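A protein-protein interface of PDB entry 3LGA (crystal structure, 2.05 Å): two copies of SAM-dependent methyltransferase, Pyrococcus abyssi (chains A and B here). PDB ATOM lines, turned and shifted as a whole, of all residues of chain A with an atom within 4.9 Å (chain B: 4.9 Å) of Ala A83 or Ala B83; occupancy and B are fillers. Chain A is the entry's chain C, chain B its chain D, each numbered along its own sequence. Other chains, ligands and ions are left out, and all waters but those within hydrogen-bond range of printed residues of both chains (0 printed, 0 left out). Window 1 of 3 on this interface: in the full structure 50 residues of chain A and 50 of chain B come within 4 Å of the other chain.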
ATOM      1  N   PRO A  79     -18.888  11.747   0.960  1.00  0.00           N
ATOM      2  CA  PRO A  79     -19.316  13.163   0.952  1.00  0.00           C
ATOM      3  C   PRO A  79     -18.212  14.204   1.125  1.00  0.00           C
ATOM      4  O   PRO A  79     -18.294  15.248   0.485  1.00  0.00           O
ATOM      5  CB  PRO A  79     -20.373  13.225   2.073  1.00  0.00           C
ATOM      6  CG  PRO A  79     -21.030  11.832   1.955  1.00  0.00           C
ATOM      7  CD  PRO A  79     -19.781  10.919   1.806  1.00  0.00           C
ATOM      8  N   LYS A  80     -17.176  13.910   1.921  1.00  0.00           N
ATOM      9  CA  LYS A  80     -16.098  14.879   2.121  1.00  0.00           C
ATOM     10  C   LYS A  80     -15.327  15.142   0.822  1.00  0.00           C
ATOM     11  O   LYS A  80     -14.806  16.240   0.606  1.00  0.00           O
ATOM     12  CB  LYS A  80     -15.122  14.408   3.210  1.00  0.00           C
ATOM     13  CG  LYS A  80     -14.114  13.314   2.728  1.00  0.00           C
ATOM     14  CD  LYS A  80     -13.200  12.838   3.822  1.00  0.00           C
ATOM     15  CE  LYS A  80     -12.449  11.544   3.371  1.00  0.00           C
ATOM     16  NZ  LYS A  80     -11.429  11.883   2.342  1.00  0.00           N
ATOM     17  N   ASP A  81     -15.235  14.126  -0.028  1.00  0.00           N
ATOM     18  CA  ASP A  81     -14.479  14.240  -1.276  1.00  0.00           C
ATOM     19  C   ASP A  81     -15.325  14.930  -2.324  1.00  0.00           C
ATOM     20  O   ASP A  81     -14.852  15.856  -2.965  1.00  0.00           O
ATOM     21  CB  ASP A  81     -14.068  12.829  -1.744  1.00  0.00           C
ATOM     22  CG  ASP A  81     -13.059  12.187  -0.794  1.00  0.00           C
ATOM     23  OD1 ASP A  81     -12.217  12.939  -0.244  1.00  0.00           O
ATOM     24  OD2 ASP A  81     -13.148  10.963  -0.567  1.00  0.00           O
ATOM     25  N   ALA A  82     -16.587  14.487  -2.469  1.00  0.00           N
ATOM     26  CA  ALA A  82     -17.606  15.209  -3.285  1.00  0.00           C
ATOM     27  C   ALA A  82     -17.716  16.676  -2.914  1.00  0.00           C
ATOM     28  O   ALA A  82     -17.850  17.530  -3.808  1.00  0.00           O
ATOM     29  CB  ALA A  82     -18.976  14.545  -3.107  1.00  0.00           C
ATOM     30  N   ALA A  83     -17.650  16.974  -1.599  1.00  0.00           N
ATOM     31  CA  ALA A  83     -17.676  18.375  -1.097  1.00  0.00           C
ATOM     32  C   ALA A  83     -16.527  19.197  -1.675  1.00  0.00           C
ATOM     33  O   ALA A  83     -16.718  20.350  -2.124  1.00  0.00           O
ATOM     34  CB  ALA A  83     -17.616  18.411   0.479  1.00  0.00           C
ATOM     35  N   LEU A  84     -15.315  18.636  -1.646  1.00  0.00           N
ATOM     36  CA  LEU A  84     -14.151  19.369  -2.172  1.00  0.00           C
ATOM     37  C   LEU A  84     -14.156  19.491  -3.694  1.00  0.00           C
ATOM     38  O   LEU A  84     -13.703  20.490  -4.240  1.00  0.00           O
ATOM     39  CB  LEU A  84     -12.824  18.783  -1.645  1.00  0.00           C
ATOM     40  CG  LEU A  84     -12.296  19.454  -0.355  1.00  0.00           C
ATOM     41  CD1 LEU A  84     -11.973  20.920  -0.555  1.00  0.00           C
ATOM     42  CD2 LEU A  84     -13.357  19.314   0.773  1.00  0.00           C
ATOM     43  N   ILE A  85     -14.677  18.473  -4.366  1.00  0.00           N
ATOM     44  CA  ILE A  85     -14.869  18.535  -5.840  1.00  0.00           C
ATOM     45  C   ILE A  85     -15.765  19.751  -6.173  1.00  0.00           C
ATOM     46  O   ILE A  85     -15.421  20.598  -6.987  1.00  0.00           O
ATOM     47  CB  ILE A  85     -15.483  17.169  -6.369  1.00  0.00           C
ATOM     48  CG1 ILE A  85     -14.412  16.088  -6.287  1.00  0.00           C
ATOM     49  CG2 ILE A  85     -16.051  17.262  -7.855  1.00  0.00           C
ATOM     50  CD1 ILE A  85     -14.952  14.645  -6.523  1.00  0.00           C
ATOM     51  N   VAL A  86     -16.910  19.848  -5.490  1.00  0.00           N
ATOM     52  CA  VAL A  86     -17.877  20.906  -5.733  1.00  0.00           C
ATOM     53  C   VAL A  86     -17.249  22.263  -5.448  1.00  0.00           C
ATOM     54  O   VAL A  86     -17.405  23.229  -6.210  1.00  0.00           O
ATOM     55  CB  VAL A  86     -19.158  20.695  -4.877  1.00  0.00           C
ATOM     56  CG1 VAL A  86     -19.950  21.981  -4.766  1.00  0.00           C
ATOM     57  CG2 VAL A  86     -20.005  19.569  -5.498  1.00  0.00           C
ATOM     58  N   ALA A  87     -16.558  22.348  -4.326  1.00  0.00           N
ATOM     59  CA  ALA A  87     -15.915  23.597  -3.917  1.00  0.00           C
ATOM     60  C   ALA A  87     -14.787  24.075  -4.831  1.00  0.00           C
ATOM     61  O   ALA A  87     -14.777  25.220  -5.271  1.00  0.00           O
ATOM     62  CB  ALA A  87     -15.424  23.471  -2.452  1.00  0.00           C
ATOM     63  N   PHE A 110     -25.063  13.428  -5.151  1.00  0.00           N
ATOM     64  CA  PHE A 110     -24.479  14.655  -4.618  1.00  0.00           C
ATOM     65  C   PHE A 110     -24.433  15.745  -5.674  1.00  0.00           C
ATOM     66  O   PHE A 110     -24.855  16.861  -5.442  1.00  0.00           O
ATOM     67  CB  PHE A 110     -23.057  14.360  -4.110  1.00  0.00           C
ATOM     68  CG  PHE A 110     -22.522  15.408  -3.165  1.00  0.00           C
ATOM     69  CD1 PHE A 110     -22.536  15.183  -1.789  1.00  0.00           C
ATOM     70  CD2 PHE A 110     -21.988  16.598  -3.648  1.00  0.00           C
ATOM     71  CE1 PHE A 110     -22.034  16.140  -0.905  1.00  0.00           C
ATOM     72  CE2 PHE A 110     -21.509  17.578  -2.774  1.00  0.00           C
ATOM     73  CZ  PHE A 110     -21.536  17.339  -1.394  1.00  0.00           C
ATOM     74  N   PRO B  79     -12.752  28.083   1.724  1.00  0.00           N
ATOM     75  CA  PRO B  79     -13.586  27.177   0.898  1.00  0.00           C
ATOM     76  C   PRO B  79     -13.706  25.737   1.387  1.00  0.00           C
ATOM     77  O   PRO B  79     -14.798  25.161   1.251  1.00  0.00           O
ATOM     78  CB  PRO B  79     -12.923  27.256  -0.492  1.00  0.00           C
ATOM     79  CG  PRO B  79     -12.471  28.734  -0.527  1.00  0.00           C
ATOM     80  CD  PRO B  79     -11.811  28.857   0.875  1.00  0.00           C
ATOM     81  N   LYS B  80     -12.636  25.167   1.958  1.00  0.00           N
ATOM     82  CA  LYS B  80     -12.708  23.789   2.458  1.00  0.00           C
ATOM     83  C   LYS B  80     -13.743  23.652   3.586  1.00  0.00           C
ATOM     84  O   LYS B  80     -14.341  22.597   3.763  1.00  0.00           O
ATOM     85  CB  LYS B  80     -11.353  23.287   2.967  1.00  0.00           C
ATOM     86  CG  LYS B  80     -10.931  23.877   4.322  1.00  0.00           C
ATOM     87  CD  LYS B  80      -9.585  23.395   4.793  1.00  0.00           C
ATOM     88  CE  LYS B  80      -9.125  24.243   6.039  1.00  0.00           C
ATOM     89  NZ  LYS B  80      -9.866  23.863   7.277  1.00  0.00           N
ATOM     90  N   ASP B  81     -13.901  24.704   4.374  1.00  0.00           N
ATOM     91  CA  ASP B  81     -14.825  24.648   5.501  1.00  0.00           C
ATOM     92  C   ASP B  81     -16.236  24.889   5.021  1.00  0.00           C
ATOM     93  O   ASP B  81     -17.128  24.174   5.428  1.00  0.00           O
ATOM     94  CB  ASP B  81     -14.420  25.689   6.543  1.00  0.00           C
ATOM     95  CG  ASP B  81     -13.069  25.363   7.158  1.00  0.00           C
ATOM     96  OD1 ASP B  81     -12.824  24.156   7.382  1.00  0.00           O
ATOM     97  OD2 ASP B  81     -12.255  26.287   7.360  1.00  0.00           O
ATOM     98  N   ALA B  82     -16.419  25.904   4.165  1.00  0.00           N
ATOM     99  CA  ALA B  82     -17.717  26.129   3.460  1.00  0.00           C
ATOM    100  C   ALA B  82     -18.171  24.889   2.715  1.00  0.00           C
ATOM    101  O   ALA B  82     -19.367  24.510   2.758  1.00  0.00           O
ATOM    102  CB  ALA B  82     -17.584  27.305   2.491  1.00  0.00           C
ATOM    103  N   ALA B  83     -17.209  24.209   2.075  1.00  0.00           N
ATOM    104  CA  ALA B  83     -17.494  22.906   1.403  1.00  0.00           C
ATOM    105  C   ALA B  83     -18.128  21.877   2.339  1.00  0.00           C
ATOM    106  O   ALA B  83     -19.108  21.219   1.974  1.00  0.00           O
ATOM    107  CB  ALA B  83     -16.205  22.303   0.788  1.00  0.00           C
ATOM    108  N   LEU B  84     -17.550  21.692   3.532  1.00  0.00           N
ATOM    109  CA  LEU B  84     -18.083  20.683   4.478  1.00  0.00           C
ATOM    110  C   LEU B  84     -19.409  21.114   5.093  1.00  0.00           C
ATOM    111  O   LEU B  84     -20.273  20.281   5.372  1.00  0.00           O
ATOM    112  CB  LEU B  84     -17.034  20.302   5.564  1.00  0.00           C
ATOM    113  CG  LEU B  84     -16.143  19.082   5.193  1.00  0.00           C
ATOM    114  CD1 LEU B  84     -16.972  17.827   5.003  1.00  0.00           C
ATOM    115  CD2 LEU B  84     -15.367  19.317   3.906  1.00  0.00           C
ATOM    116  N   ILE B  85     -19.577  22.417   5.262  1.00  0.00           N
ATOM    117  CA  ILE B  85     -20.872  22.975   5.740  1.00  0.00           C
ATOM    118  C   ILE B  85     -21.968  22.584   4.740  1.00  0.00           C
ATOM    119  O   ILE B  85     -22.998  22.008   5.103  1.00  0.00           O
ATOM    120  CB  ILE B  85     -20.793  24.546   5.921  1.00  0.00           C
ATOM    121  CG1 ILE B  85     -19.910  24.857   7.126  1.00  0.00           C
ATOM    122  CG2 ILE B  85     -22.238  25.188   6.085  1.00  0.00           C
ATOM    123  CD1 ILE B  85     -19.503  26.346   7.274  1.00  0.00           C
ATOM    124  N   VAL B  86     -21.711  22.843   3.457  1.00  0.00           N
ATOM    125  CA  VAL B  86     -22.674  22.555   2.410  1.00  0.00           C
ATOM    126  C   VAL B  86     -22.990  21.068   2.359  1.00  0.00           C
ATOM    127  O   VAL B  86     -24.164  20.647   2.280  1.00  0.00           O
ATOM    128  CB  VAL B  86     -22.171  23.121   1.032  1.00  0.00           C
ATOM    129  CG1 VAL B  86     -22.897  22.444  -0.141  1.00  0.00           C
ATOM    130  CG2 VAL B  86     -22.406  24.658   1.012  1.00  0.00           C
ATOM    131  N   ALA B  87     -21.937  20.262   2.413  1.00  0.00           N
ATOM    132  CA  ALA B  87     -22.047  18.814   2.315  1.00  0.00           C
ATOM    133  C   ALA B  87     -22.780  18.167   3.489  1.00  0.00           C
ATOM    134  O   ALA B  87     -23.716  17.387   3.293  1.00  0.00           O
ATOM    135  CB  ALA B  87     -20.647  18.210   2.138  1.00  0.00           C
ATOM    136  N   PHE B 110     -20.162  31.920  -1.258  1.00  0.00           N
ATOM    137  CA  PHE B 110     -20.192  30.466  -1.439  1.00  0.00           C
ATOM    138  C   PHE B 110     -21.604  29.927  -1.312  1.00  0.00           C
ATOM    139  O   PHE B 110     -22.073  29.185  -2.153  1.00  0.00           O
ATOM    140  CB  PHE B 110     -19.300  29.824  -0.385  1.00  0.00           C
ATOM    141  CG  PHE B 110     -18.889  28.418  -0.727  1.00  0.00           C
ATOM    142  CD1 PHE B 110     -17.634  28.176  -1.294  1.00  0.00           C
ATOM    143  CD2 PHE B 110     -19.749  27.351  -0.486  1.00  0.00           C
ATOM    144  CE1 PHE B 110     -17.237  26.880  -1.620  1.00  0.00           C
ATOM    145  CE2 PHE B 110     -19.386  26.033  -0.817  1.00  0.00           C
ATOM    146  CZ  PHE B 110     -18.117  25.797  -1.382  1.00  0.00           C
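CB of Ala A83 touches O of Ala B83, at 3.5 Å.
Ala B87 touches Ala A83 (CB to CB, 3.5 Å).
Leu A84 touches Leu B84 (CD2 to CD2, 3.7 Å).
CB of Ala A87 touches CB of Ala B83, at 3.5 Å.
CB of Ala A87 touches CZ of Phe B110, at 3.7 Å.
Ala B87 touches Phe A110.
Ala A83 touches two residues of chain B.
Printed residues of chain B within 4 Å of Ala A87: Ala B83 (3.5 Å) and Phe B110 (3.7 Å).
Printed residues of chain B within 4 Å of Phe A110: Ala B87.
Pro B79 touches none of the printed residues of chain A.
Of the printed residues of chain A, Ala B83 touches Ala A83 and Ala A87.
Printed residues of chain A within 4 Å of Ala B87: Ala A83 (3.5 Å) and Phe A110 (3.7 Å).
The nearest residue of chain B that does not touch Ala A83 is Leu B84 (4.2 Å).
The nearest residue of chain A that does not touch Ala B83 is Leu A84 (4.1 Å).
The nearest printed residue of chain B that does not touch Leu A84 is Ala B83 (4.1 Å).
Hydrophobic or aromatic side chains of chain B that line the printed part of chain A: Ala B83, Leu B84, Ala B87 and Phe B110.
Of the 10 printed residues of chain A, 4 touch a printed residue of chain B.
Hydrophobic or aromatic side chains of chain A within 4 Å of the printed part of chain B: Ala A83, Leu A84, Ala A87 and Phe A110.
Among the printed residues, no Asp or Glu carboxylate lies within 4 Å of a Lys or Arg side-chain nitrogen of the other chain.
Ala B83 touches its own counterpart, Ala A83.
Ala A83 touches Ala B87, and with the chains exchanged Ala A87 touches Ala B83.
Leu B84 touches its own counterpart, Leu A84.
Ala A87 touches Phe B110, and with the chains exchanged Phe A110 touches Ala B87.
Positions printed for both chains: 79, 80, 81, 82, 83, 84, 85, 86, 87 and 110.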
